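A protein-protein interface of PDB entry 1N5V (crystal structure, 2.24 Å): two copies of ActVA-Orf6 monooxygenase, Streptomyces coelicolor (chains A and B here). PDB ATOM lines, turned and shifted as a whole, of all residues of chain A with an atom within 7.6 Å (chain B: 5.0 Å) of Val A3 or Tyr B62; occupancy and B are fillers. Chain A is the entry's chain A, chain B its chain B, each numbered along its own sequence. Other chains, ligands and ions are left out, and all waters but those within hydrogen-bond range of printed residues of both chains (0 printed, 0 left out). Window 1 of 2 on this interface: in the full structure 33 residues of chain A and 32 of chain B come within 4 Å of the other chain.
Printed residues of chain A that touch a printed residue of chain B: Ala A1, Glu A2, Val A3, Val A11, Thr A49, His A51, Tyr A62, Gln A64, Met A103, Pro A105, Gly A107, Ala A108 and Ile A109. Hydrophobic or aromatic side chains of chain A within 4 Å of the printed part of chain B: Val A3, Val A11, His A51, Tyr A62, Met A103, Pro A105 and Ala A108. Of the 14 printed residues of chain B, 10 touch a printed residue of chain A. Printed residues of chain B that touch a printed residue of chain A: Ala B1, Val B3, Val B11, Ser B47, Ala B48, Thr B49, His B51, Val B60, Tyr B62 and Gln B64. Hydrophobic or aromatic side chains of chain B within 4 Å of the printed part of chain A: Val B3, Val B11, His B51, Val B60 and Tyr B62. Among the printed residues, no Asp or Glu carboxylate lies within 4 Å of a Lys or Arg side-chain nitrogen of the other chain.
Among the printed residues, merely in contact across the chains: Ala A1 with Val B3, Val A3 with Val B3, Val A3 with Ser B47, Val A3 with Thr B49, Val A3 with Tyr B62, Val A3 with Gln B64, Val A11 with His B51, Thr A49 with Val B3, His A51 with Val B11, Tyr A62 with Tyr B62, Gln A64 with Val B3, Met A103 with His B51, Met A103 with Val B60, Pro A105 with His B51, Gly A107 with Thr B49, Ala A108 with Ala B48 and Ile A109 with Ser B47.
Val A3 touches Thr B49, and with the chains exchanged Thr A49 touches Val B3. Val A3 touches Tyr B62, but with the chains exchanged Tyr A62 does not touch Val B3 (4.4 Å). Val A3 touches Gln B64, and with the chains exchanged Gln A64 touches Val B3. Val A11 touches His B51, and with the chains exchanged His A51 touches Val B11.
Of the printed residues of chain B, Glu A2 touches Ala B1. Printed residues of chain B within 4 Å of Val A3: Ala B1 (3.4 Å), Val B3 (3.9 Å), Ser B47 (3.8 Å), Thr B49 (3.5 Å), Tyr B62 (3.996 Å) and Gln B64 (3.8 Å). Of the printed residues of chain A, Ala B48 touches Ala A108 (3.2 Å) and Ile A109 (2.9 Å). Of the printed residues of chain A, Tyr B62 touches Val A3, His A51 and Tyr A62. The nearest printed residue of chain B that does not touch Glu A2 is Val B3 (5.2 Å).
The side-chain hydroxyl (OH) of Tyr A62 sits at hydrogen-bond distance from a ring nitrogen (NE2) of His B51. The backbone NH (N) of Ile A109 sits at hydrogen-bond distance from the backbone carbonyl oxygen (O) of Ala B48, at 2.9 Å. The backbone NH of Val A3 is in hydrogen-bond range of the backbone carbonyl oxygen of Ala B1. OE1 of Glu A2 sits at hydrogen-bond distance from N of Ala B1, at 3.0 Å. OH of Tyr B62 sits at hydrogen-bond distance from NE2 of His A51 (2.7 Å).
The backbone NH (N) of Thr A49 sits at hydrogen-bond distance from the backbone carbonyl oxygen (O) of Tyr A62, at 2.9 Å. The backbone NH (N) of His B51 lies within hydrogen-bond range of the backbone carbonyl oxygen (O) of Val B60 (2.7 Å). N of Thr B49 is in hydrogen-bond range of OD1 of Asn B61. The backbone carbonyl oxygen (O) of Thr A49 is in hydrogen-bond range of a ring nitrogen (ND1) of His A51 (3.2 Å). N of Ala B1 sits at hydrogen-bond distance from OE1 of Gln B64, at 3.3 Å. O of Thr B49 lies within hydrogen-bond range of N of Tyr B62, 2.9 Å away.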
ATOM      1  N   ALA A   1      21.885  28.316 -10.165  1.00  0.00           N
ATOM      2  CA  ALA A   1      21.141  28.866 -11.320  1.00  0.00           C
ATOM      3  C   ALA A   1      19.968  28.005 -11.787  1.00  0.00           C
ATOM      4  O   ALA A   1      19.885  26.821 -11.471  1.00  0.00           O
ATOM      5  CB  ALA A   1      22.133  29.004 -12.463  1.00  0.00           C
ATOM      6  N   GLU A   2      19.034  28.596 -12.544  1.00  0.00           N
ATOM      7  CA  GLU A   2      17.986  27.750 -13.116  1.00  0.00           C
ATOM      8  C   GLU A   2      18.732  26.622 -13.840  1.00  0.00           C
ATOM      9  O   GLU A   2      19.836  26.834 -14.357  1.00  0.00           O
ATOM     10  CB  GLU A   2      17.074  28.522 -14.049  1.00  0.00           C
ATOM     11  CG  GLU A   2      15.746  28.866 -13.379  1.00  0.00           C
ATOM     12  CD  GLU A   2      14.692  27.785 -13.606  1.00  0.00           C
ATOM     13  OE1 GLU A   2      14.979  26.763 -14.287  1.00  0.00           O
ATOM     14  OE2 GLU A   2      13.566  27.957 -13.071  1.00  0.00           O
ATOM     15  N   VAL A   3      18.137  25.435 -13.855  1.00  0.00           N
ATOM     16  CA  VAL A   3      18.766  24.279 -14.445  1.00  0.00           C
ATOM     17  C   VAL A   3      18.951  24.379 -15.952  1.00  0.00           C
ATOM     18  O   VAL A   3      19.682  23.605 -16.546  1.00  0.00           O
ATOM     19  CB  VAL A   3      17.959  22.981 -14.173  1.00  0.00           C
ATOM     20  CG1 VAL A   3      18.275  22.431 -12.799  1.00  0.00           C
ATOM     21  CG2 VAL A   3      16.472  23.214 -14.336  1.00  0.00           C
ATOM     22  N   ASN A   4      18.136  25.231 -16.559  1.00  0.00           N
ATOM     23  CA  ASN A   4      18.092  25.414 -17.999  1.00  0.00           C
ATOM     24  C   ASN A   4      18.757  26.718 -18.403  1.00  0.00           C
ATOM     25  O   ASN A   4      18.637  27.135 -19.546  1.00  0.00           O
ATOM     26  CB  ASN A   4      16.616  25.416 -18.450  1.00  0.00           C
ATOM     27  CG  ASN A   4      15.860  26.557 -17.805  1.00  0.00           C
ATOM     28  OD1 ASN A   4      15.996  26.749 -16.587  1.00  0.00           O
ATOM     29  ND2 ASN A   4      15.069  27.305 -18.568  1.00  0.00           N
ATOM     30  N   ASP A   5      19.405  27.391 -17.465  1.00  0.00           N
ATOM     31  CA  ASP A   5      20.065  28.648 -17.794  1.00  0.00           C
ATOM     32  C   ASP A   5      21.198  28.453 -18.795  1.00  0.00           C
ATOM     33  O   ASP A   5      22.148  27.713 -18.552  1.00  0.00           O
ATOM     34  CB  ASP A   5      20.629  29.244 -16.508  1.00  0.00           C
ATOM     35  CG  ASP A   5      21.224  30.629 -16.665  1.00  0.00           C
ATOM     36  OD1 ASP A   5      21.341  31.067 -17.834  1.00  0.00           O
ATOM     37  OD2 ASP A   5      21.557  31.221 -15.607  1.00  0.00           O
ATOM     38  N   PRO A   6      21.181  29.237 -19.874  1.00  0.00           N
ATOM     39  CA  PRO A   6      22.220  29.216 -20.888  1.00  0.00           C
ATOM     40  C   PRO A   6      23.607  29.607 -20.415  1.00  0.00           C
ATOM     41  O   PRO A   6      24.552  29.252 -21.132  1.00  0.00           O
ATOM     42  CB  PRO A   6      21.694  30.105 -22.010  1.00  0.00           C
ATOM     43  CG  PRO A   6      20.221  30.176 -21.765  1.00  0.00           C
ATOM     44  CD  PRO A   6      20.087  30.171 -20.256  1.00  0.00           C
ATOM     45  N   VAL A   8      24.952  28.117 -17.875  1.00  0.00           N
ATOM     46  CA  VAL A   8      25.492  26.853 -17.393  1.00  0.00           C
ATOM     47  C   VAL A   8      26.238  26.156 -18.539  1.00  0.00           C
ATOM     48  O   VAL A   8      25.708  25.498 -19.419  1.00  0.00           O
ATOM     49  CB  VAL A   8      24.428  25.925 -16.773  1.00  0.00           C
ATOM     50  CG1 VAL A   8      25.049  24.608 -16.335  1.00  0.00           C
ATOM     51  CG2 VAL A   8      23.748  26.577 -15.567  1.00  0.00           C
ATOM     52  N   VAL A  11      28.804  20.869 -16.122  1.00  0.00           N
ATOM     53  CA  VAL A  11      28.233  20.186 -14.994  1.00  0.00           C
ATOM     54  C   VAL A  11      29.114  19.024 -14.599  1.00  0.00           C
ATOM     55  O   VAL A  11      29.563  18.174 -15.366  1.00  0.00           O
ATOM     56  CB  VAL A  11      26.798  19.717 -15.354  1.00  0.00           C
ATOM     57  CG1 VAL A  11      26.176  18.805 -14.285  1.00  0.00           C
ATOM     58  CG2 VAL A  11      25.859  20.899 -15.589  1.00  0.00           C
ATOM     59  N   VAL A  13      28.732  15.861 -11.877  1.00  0.00           N
ATOM     60  CA  VAL A  13      27.828  15.073 -11.046  1.00  0.00           C
ATOM     61  C   VAL A  13      28.751  14.145 -10.271  1.00  0.00           C
ATOM     62  O   VAL A  13      29.387  13.280 -10.852  1.00  0.00           O
ATOM     63  CB  VAL A  13      26.853  14.270 -11.909  1.00  0.00           C
ATOM     64  CG1 VAL A  13      26.022  13.372 -11.010  1.00  0.00           C
ATOM     65  CG2 VAL A  13      25.998  15.211 -12.743  1.00  0.00           C
ATOM     66  N   THR A  49      24.697  21.383  -5.483  1.00  0.00           N
ATOM     67  CA  THR A  49      23.546  20.869  -4.708  1.00  0.00           C
ATOM     68  C   THR A  49      23.714  19.424  -4.272  1.00  0.00           C
ATOM     69  O   THR A  49      23.976  18.582  -5.125  1.00  0.00           O
ATOM     70  CB  THR A  49      22.270  20.976  -5.529  1.00  0.00           C
ATOM     71  OG1 THR A  49      22.184  22.378  -5.869  1.00  0.00           O
ATOM     72  CG2 THR A  49      21.047  20.509  -4.777  1.00  0.00           C
ATOM     73  N   TYR A  50      23.684  19.188  -2.975  1.00  0.00           N
ATOM     74  CA  TYR A  50      23.951  17.862  -2.419  1.00  0.00           C
ATOM     75  C   TYR A  50      22.645  17.148  -2.078  1.00  0.00           C
ATOM     76  O   TYR A  50      21.752  17.701  -1.438  1.00  0.00           O
ATOM     77  CB  TYR A  50      24.732  17.932  -1.114  1.00  0.00           C
ATOM     78  CG  TYR A  50      26.179  18.290  -1.398  1.00  0.00           C
ATOM     79  CD1 TYR A  50      26.487  19.631  -1.628  1.00  0.00           C
ATOM     80  CD2 TYR A  50      27.153  17.351  -1.442  1.00  0.00           C
ATOM     81  CE1 TYR A  50      27.795  19.998  -1.924  1.00  0.00           C
ATOM     82  CE2 TYR A  50      28.465  17.678  -1.754  1.00  0.00           C
ATOM     83  CZ  TYR A  50      28.749  19.010  -1.997  1.00  0.00           C
ATOM     84  OH  TYR A  50      30.034  19.383  -2.223  1.00  0.00           O
ATOM     85  N   HIS A  51      22.567  15.909  -2.544  1.00  0.00           N
ATOM     86  CA  HIS A  51      21.317  15.200  -2.365  1.00  0.00           C
ATOM     87  C   HIS A  51      21.635  13.867  -1.686  1.00  0.00           C
ATOM     88  O   HIS A  51      22.648  13.246  -2.067  1.00  0.00           O
ATOM     89  CB  HIS A  51      20.804  14.875  -3.780  1.00  0.00           C
ATOM     90  CG  HIS A  51      20.596  15.925  -4.805  1.00  0.00           C
ATOM     91  ND1 HIS A  51      21.592  16.507  -5.570  1.00  0.00           N
ATOM     92  CD2 HIS A  51      19.411  16.455  -5.279  1.00  0.00           C
ATOM     93  CE1 HIS A  51      21.048  17.373  -6.406  1.00  0.00           C
ATOM     94  NE2 HIS A  51      19.701  17.358  -6.243  1.00  0.00           N
ATOM     95  N   VAL A  60      24.917  12.632  -3.683  1.00  0.00           N
ATOM     96  CA  VAL A  60      25.221  13.080  -5.035  1.00  0.00           C
ATOM     97  C   VAL A  60      25.267  14.598  -5.109  1.00  0.00           C
ATOM     98  O   VAL A  60      24.338  15.286  -4.675  1.00  0.00           O
ATOM     99  CB  VAL A  60      24.143  12.589  -5.999  1.00  0.00           C
ATOM    100  CG1 VAL A  60      24.444  13.093  -7.422  1.00  0.00           C
ATOM    101  CG2 VAL A  60      24.041  11.061  -6.021  1.00  0.00           C
ATOM    102  N   ASN A  61      26.296  15.191  -5.635  1.00  0.00           N
ATOM    103  CA  ASN A  61      26.435  16.636  -5.829  1.00  0.00           C
ATOM    104  C   ASN A  61      26.201  16.913  -7.334  1.00  0.00           C
ATOM    105  O   ASN A  61      26.917  16.327  -8.113  1.00  0.00           O
ATOM    106  CB  ASN A  61      27.893  17.024  -5.520  1.00  0.00           C
ATOM    107  CG  ASN A  61      28.279  18.462  -5.786  1.00  0.00           C
ATOM    108  OD1 ASN A  61      27.463  19.338  -5.929  1.00  0.00           O
ATOM    109  ND2 ASN A  61      29.547  18.881  -5.751  1.00  0.00           N
ATOM    110  N   TYR A  62      25.284  17.734  -7.745  1.00  0.00           N
ATOM    111  CA  TYR A  62      25.013  18.243  -9.065  1.00  0.00           C
ATOM    112  C   TYR A  62      25.566  19.669  -9.045  1.00  0.00           C
ATOM    113  O   TYR A  62      25.025  20.471  -8.269  1.00  0.00           O
ATOM    114  CB  TYR A  62      23.513  18.317  -9.378  1.00  0.00           C
ATOM    115  CG  TYR A  62      23.169  18.841 -10.746  1.00  0.00           C
ATOM    116  CD1 TYR A  62      23.297  18.038 -11.871  1.00  0.00           C
ATOM    117  CD2 TYR A  62      22.727  20.149 -10.924  1.00  0.00           C
ATOM    118  CE1 TYR A  62      23.002  18.494 -13.185  1.00  0.00           C
ATOM    119  CE2 TYR A  62      22.452  20.647 -12.194  1.00  0.00           C
ATOM    120  CZ  TYR A  62      22.598  19.805 -13.287  1.00  0.00           C
ATOM    121  OH  TYR A  62      22.353  20.315 -14.528  1.00  0.00           O
ATOM    122  N   ALA A  63      26.723  19.872  -9.638  1.00  0.00           N
ATOM    123  CA  ALA A  63      27.442  21.130  -9.595  1.00  0.00           C
ATOM    124  C   ALA A  63      27.420  21.837 -10.945  1.00  0.00           C
ATOM    125  O   ALA A  63      27.636  21.261 -12.039  1.00  0.00           O
ATOM    126  CB  ALA A  63      28.842  20.850  -9.102  1.00  0.00           C
ATOM    127  N   GLN A  64      27.088  23.105 -10.941  1.00  0.00           N
ATOM    128  CA  GLN A  64      26.945  23.920 -12.156  1.00  0.00           C
ATOM    129  C   GLN A  64      28.090  24.926 -12.253  1.00  0.00           C
ATOM    130  O   GLN A  64      28.427  25.533 -11.237  1.00  0.00           O
ATOM    131  CB  GLN A  64      25.644  24.738 -12.070  1.00  0.00           C
ATOM    132  CG  GLN A  64      24.337  24.031 -12.300  1.00  0.00           C
ATOM    133  CD  GLN A  64      23.118  24.908 -12.010  1.00  0.00           C
ATOM    134  OE1 GLN A  64      23.141  25.775 -11.109  1.00  0.00           O
ATOM    135  NE2 GLN A  64      22.001  24.722 -12.713  1.00  0.00           N
ATOM    136  N   MET A 103      29.953  16.668 -17.954  1.00  0.00           N
ATOM    137  CA  MET A 103      28.953  16.814 -18.948  1.00  0.00           C
ATOM    138  C   MET A 103      28.521  18.234 -19.190  1.00  0.00           C
ATOM    139  O   MET A 103      28.627  19.194 -18.413  1.00  0.00           O
ATOM    140  CB  MET A 103      27.754  15.941 -18.402  1.00  0.00           C
ATOM    141  CG  MET A 103      27.065  16.502 -17.200  1.00  0.00           C
ATOM    142  SD  MET A 103      25.730  15.493 -16.494  1.00  0.00           S
ATOM    143  CE  MET A 103      26.595  14.010 -16.062  1.00  0.00           C
ATOM    144  N   PRO A 105      25.094  20.595 -20.429  1.00  0.00           N
ATOM    145  CA  PRO A 105      23.655  20.643 -20.610  1.00  0.00           C
ATOM    146  C   PRO A 105      23.329  20.710 -22.108  1.00  0.00           C
ATOM    147  O   PRO A 105      24.086  21.412 -22.772  1.00  0.00           O
ATOM    148  CB  PRO A 105      23.191  21.836 -19.818  1.00  0.00           C
ATOM    149  CG  PRO A 105      24.360  22.424 -19.120  1.00  0.00           C
ATOM    150  CD  PRO A 105      25.587  21.739 -19.660  1.00  0.00           C
ATOM    151  N   ARG A 106      22.344  19.969 -22.610  1.00  0.00           N
ATOM    152  CA  ARG A 106      22.026  20.005 -24.033  1.00  0.00           C
ATOM    153  C   ARG A 106      20.587  20.448 -24.328  1.00  0.00           C
ATOM    154  O   ARG A 106      20.399  21.423 -25.055  1.00  0.00           O
ATOM    155  CB  ARG A 106      22.298  18.700 -24.765  1.00  0.00           C
ATOM    156  CG  ARG A 106      23.690  18.450 -25.245  1.00  0.00           C
ATOM    157  CD  ARG A 106      24.277  19.510 -26.176  1.00  0.00           C
ATOM    158  NE  ARG A 106      25.731  19.544 -26.143  1.00  0.00           N
ATOM    159  CZ  ARG A 106      26.702  20.407 -26.342  1.00  0.00           C
ATOM    160  NH1 ARG A 106      26.511  21.681 -26.674  1.00  0.00           N
ATOM    161  NH2 ARG A 106      27.975  20.026 -26.194  1.00  0.00           N
ATOM    162  N   GLY A 107      19.570  19.828 -23.771  1.00  0.00           N
ATOM    163  CA  GLY A 107      18.171  20.149 -23.931  1.00  0.00           C
ATOM    164  C   GLY A 107      17.489  20.097 -22.547  1.00  0.00           C
ATOM    165  O   GLY A 107      18.017  19.576 -21.538  1.00  0.00           O
ATOM    166  N   ALA A 108      16.314  20.706 -22.491  1.00  0.00           N
ATOM    167  CA  ALA A 108      15.507  20.828 -21.309  1.00  0.00           C
ATOM    168  C   ALA A 108      14.033  21.090 -21.614  1.00  0.00           C
ATOM    169  O   ALA A 108      13.583  21.748 -22.553  1.00  0.00           O
ATOM    170  CB  ALA A 108      15.989  21.972 -20.420  1.00  0.00           C
ATOM    171  N   ILE A 109      13.249  20.484 -20.739  1.00  0.00           N
ATOM    172  CA  ILE A 109      11.793  20.554 -20.713  1.00  0.00           C
ATOM    173  C   ILE A 109      11.411  21.296 -19.439  1.00  0.00           C
ATOM    174  O   ILE A 109      11.802  20.824 -18.365  1.00  0.00           O
ATOM    175  CB  ILE A 109      11.268  19.107 -20.719  1.00  0.00           C
ATOM    176  CG1 ILE A 109      11.796  18.350 -21.934  1.00  0.00           C
ATOM    177  CG2 ILE A 109       9.746  19.110 -20.685  1.00  0.00           C
ATOM    178  CD1 ILE A 109      11.199  16.987 -22.249  1.00  0.00           C
ATOM    179  N   LEU A 110      10.846  22.479 -19.480  1.00  0.00           N
ATOM    180  CA  LEU A 110      10.417  23.262 -18.338  1.00  0.00           C
ATOM    181  C   LEU A 110       8.895  23.257 -18.305  1.00  0.00           C
ATOM    182  O   LEU A 110       8.239  22.871 -19.266  1.00  0.00           O
ATOM    183  CB  LEU A 110      11.154  24.588 -18.210  1.00  0.00           C
ATOM    184  CG  LEU A 110      12.376  24.475 -17.245  1.00  0.00           C
ATOM    185  CD1 LEU A 110      13.589  23.850 -17.899  1.00  0.00           C
ATOM    186  CD2 LEU A 110      12.792  25.776 -16.607  1.00  0.00           C
ATOM    187  N   ALA B   1      13.494  24.853 -12.565  1.00  0.00           N
ATOM    188  CA  ALA B   1      13.515  25.585 -11.257  1.00  0.00           C
ATOM    189  C   ALA B   1      14.965  25.766 -10.795  1.00  0.00           C
ATOM    190  O   ALA B   1      15.883  25.148 -11.335  1.00  0.00           O
ATOM    191  CB  ALA B   1      12.699  24.789 -10.234  1.00  0.00           C
ATOM    192  N   VAL B   3      18.103  25.294  -8.525  1.00  0.00           N
ATOM    193  CA  VAL B   3      18.552  24.053  -7.905  1.00  0.00           C
ATOM    194  C   VAL B   3      18.161  23.968  -6.442  1.00  0.00           C
ATOM    195  O   VAL B   3      17.818  22.877  -5.954  1.00  0.00           O
ATOM    196  CB  VAL B   3      20.075  23.850  -8.116  1.00  0.00           C
ATOM    197  CG1 VAL B   3      20.220  23.458  -9.572  1.00  0.00           C
ATOM    198  CG2 VAL B   3      20.879  25.081  -7.692  1.00  0.00           C
ATOM    199  N   VAL B  11      14.268  14.285  -6.825  1.00  0.00           N
ATOM    200  CA  VAL B  11      15.009  14.325  -8.082  1.00  0.00           C
ATOM    201  C   VAL B  11      15.240  12.959  -8.721  1.00  0.00           C
ATOM    202  O   VAL B  11      15.553  11.980  -8.024  1.00  0.00           O
ATOM    203  CB  VAL B  11      16.420  14.982  -7.798  1.00  0.00           C
ATOM    204  CG1 VAL B  11      17.375  14.844  -8.982  1.00  0.00           C
ATOM    205  CG2 VAL B  11      16.204  16.453  -7.445  1.00  0.00           C
ATOM    206  N   ALA B  12      15.199  12.839 -10.040  1.00  0.00           N
ATOM    207  CA  ALA B  12      15.556  11.577 -10.713  1.00  0.00           C
ATOM    208  C   ALA B  12      16.722  11.922 -11.659  1.00  0.00           C
ATOM    209  O   ALA B  12      16.680  12.958 -12.335  1.00  0.00           O
ATOM    210  CB  ALA B  12      14.460  10.928 -11.507  1.00  0.00           C
ATOM    211  N   VAL B  13      17.814  11.199 -11.506  1.00  0.00           N
ATOM    212  CA  VAL B  13      18.998  11.353 -12.346  1.00  0.00           C
ATOM    213  C   VAL B  13      19.073  10.041 -13.151  1.00  0.00           C
ATOM    214  O   VAL B  13      19.233   8.956 -12.567  1.00  0.00           O
ATOM    215  CB  VAL B  13      20.257  11.556 -11.519  1.00  0.00           C
ATOM    216  CG1 VAL B  13      21.494  11.353 -12.409  1.00  0.00           C
ATOM    217  CG2 VAL B  13      20.327  12.954 -10.916  1.00  0.00           C
ATOM    218  N   SER B  47      11.062  19.928 -13.827  1.00  0.00           N
ATOM    219  CA  SER B  47      11.988  20.138 -14.947  1.00  0.00           C
ATOM    220  C   SER B  47      12.706  18.836 -15.290  1.00  0.00           C
ATOM    221  O   SER B  47      12.663  17.913 -14.470  1.00  0.00           O
ATOM    222  CB  SER B  47      13.153  21.076 -14.589  1.00  0.00           C
ATOM    223  OG  SER B  47      14.073  20.266 -13.824  1.00  0.00           O
ATOM    224  N   ALA B  48      13.198  18.777 -16.513  1.00  0.00           N
ATOM    225  CA  ALA B  48      13.992  17.646 -16.952  1.00  0.00           C
ATOM    226  C   ALA B  48      15.087  18.347 -17.780  1.00  0.00           C
ATOM    227  O   ALA B  48      14.758  19.143 -18.658  1.00  0.00           O
ATOM    228  CB  ALA B  48      13.279  16.588 -17.717  1.00  0.00           C
ATOM    229  N   THR B  49      16.343  18.149 -17.394  1.00  0.00           N
ATOM    230  CA  THR B  49      17.442  18.740 -18.144  1.00  0.00           C
ATOM    231  C   THR B  49      18.339  17.606 -18.669  1.00  0.00           C
ATOM    232  O   THR B  49      18.790  16.778 -17.893  1.00  0.00           O
ATOM    233  CB  THR B  49      18.234  19.671 -17.237  1.00  0.00           C
ATOM    234  OG1 THR B  49      17.332  20.634 -16.674  1.00  0.00           O
ATOM    235  CG2 THR B  49      19.361  20.384 -17.982  1.00  0.00           C
ATOM    236  N   HIS B  51      21.712  16.175 -20.522  1.00  0.00           N
ATOM    237  CA  HIS B  51      23.125  16.514 -20.747  1.00  0.00           C
ATOM    238  C   HIS B  51      23.874  15.448 -21.542  1.00  0.00           C
ATOM    239  O   HIS B  51      23.651  14.273 -21.397  1.00  0.00           O
ATOM    240  CB  HIS B  51      23.909  16.620 -19.435  1.00  0.00           C
ATOM    241  CG  HIS B  51      23.221  17.316 -18.298  1.00  0.00           C
ATOM    242  ND1 HIS B  51      22.101  16.776 -17.647  1.00  0.00           N
ATOM    243  CD2 HIS B  51      23.499  18.505 -17.704  1.00  0.00           C
ATOM    244  CE1 HIS B  51      21.736  17.610 -16.706  1.00  0.00           C
ATOM    245  NE2 HIS B  51      22.581  18.638 -16.704  1.00  0.00           N
ATOM    246  N   VAL B  60      22.581  12.234 -19.693  1.00  0.00           N
ATOM    247  CA  VAL B  60      22.106  12.197 -18.302  1.00  0.00           C
ATOM    248  C   VAL B  60      20.977  13.230 -18.161  1.00  0.00           C
ATOM    249  O   VAL B  60      21.029  14.365 -18.631  1.00  0.00           O
ATOM    250  CB  VAL B  60      23.235  12.506 -17.307  1.00  0.00           C
ATOM    251  CG1 VAL B  60      22.696  12.532 -15.895  1.00  0.00           C
ATOM    252  CG2 VAL B  60      24.458  11.595 -17.475  1.00  0.00           C
ATOM    253  N   ASN B  61      19.874  12.751 -17.618  1.00  0.00           N
ATOM    254  CA  ASN B  61      18.730  13.653 -17.363  1.00  0.00           C
ATOM    255  C   ASN B  61      18.752  13.973 -15.865  1.00  0.00           C
ATOM    256  O   ASN B  61      18.638  13.010 -15.071  1.00  0.00           O
ATOM    257  CB  ASN B  61      17.412  12.984 -17.792  1.00  0.00           C
ATOM    258  CG  ASN B  61      16.137  13.748 -17.472  1.00  0.00           C
ATOM    259  OD1 ASN B  61      16.138  14.944 -17.140  1.00  0.00           O
ATOM    260  ND2 ASN B  61      14.988  13.060 -17.552  1.00  0.00           N
ATOM    261  N   TYR B  62      18.746  15.243 -15.479  1.00  0.00           N
ATOM    262  CA  TYR B  62      18.658  15.604 -14.042  1.00  0.00           C
ATOM    263  C   TYR B  62      17.208  16.095 -13.913  1.00  0.00           C
ATOM    264  O   TYR B  62      16.903  17.046 -14.676  1.00  0.00           O
ATOM    265  CB  TYR B  62      19.599  16.708 -13.627  1.00  0.00           C
ATOM    266  CG  TYR B  62      19.396  17.310 -12.246  1.00  0.00           C
ATOM    267  CD1 TYR B  62      18.598  18.465 -12.034  1.00  0.00           C
ATOM    268  CD2 TYR B  62      20.003  16.707 -11.158  1.00  0.00           C
ATOM    269  CE1 TYR B  62      18.457  18.991 -10.773  1.00  0.00           C
ATOM    270  CE2 TYR B  62      19.832  17.247  -9.880  1.00  0.00           C
ATOM    271  CZ  TYR B  62      19.050  18.367  -9.678  1.00  0.00           C
ATOM    272  OH  TYR B  62      18.912  18.857  -8.369  1.00  0.00           O
ATOM    273  N   ALA B  63      16.297  15.328 -13.277  1.00  0.00           N
ATOM    274  CA  ALA B  63      14.893  15.825 -13.304  1.00  0.00           C
ATOM    275  C   ALA B  63      14.361  16.240 -11.934  1.00  0.00           C
ATOM    276  O   ALA B  63      14.502  15.466 -10.971  1.00  0.00           O
ATOM    277  CB  ALA B  63      13.993  14.751 -13.902  1.00  0.00           C
ATOM    278  N   GLN B  64      13.703  17.374 -11.876  1.00  0.00           N
ATOM    279  CA  GLN B  64      13.175  17.922 -10.632  1.00  0.00           C
ATOM    280  C   GLN B  64      11.671  17.776 -10.426  1.00  0.00           C
ATOM    281  O   GLN B  64      10.886  18.065 -11.311  1.00  0.00           O
ATOM    282  CB  GLN B  64      13.422  19.429 -10.537  1.00  0.00           C
ATOM    283  CG  GLN B  64      14.912  19.796 -10.407  1.00  0.00           C
ATOM    284  CD  GLN B  64      14.981  21.306 -10.661  1.00  0.00           C
ATOM    285  OE1 GLN B  64      14.307  21.839 -11.556  1.00  0.00           O
ATOM    286  NE2 GLN B  64      15.765  22.019  -9.898  1.00  0.00           N
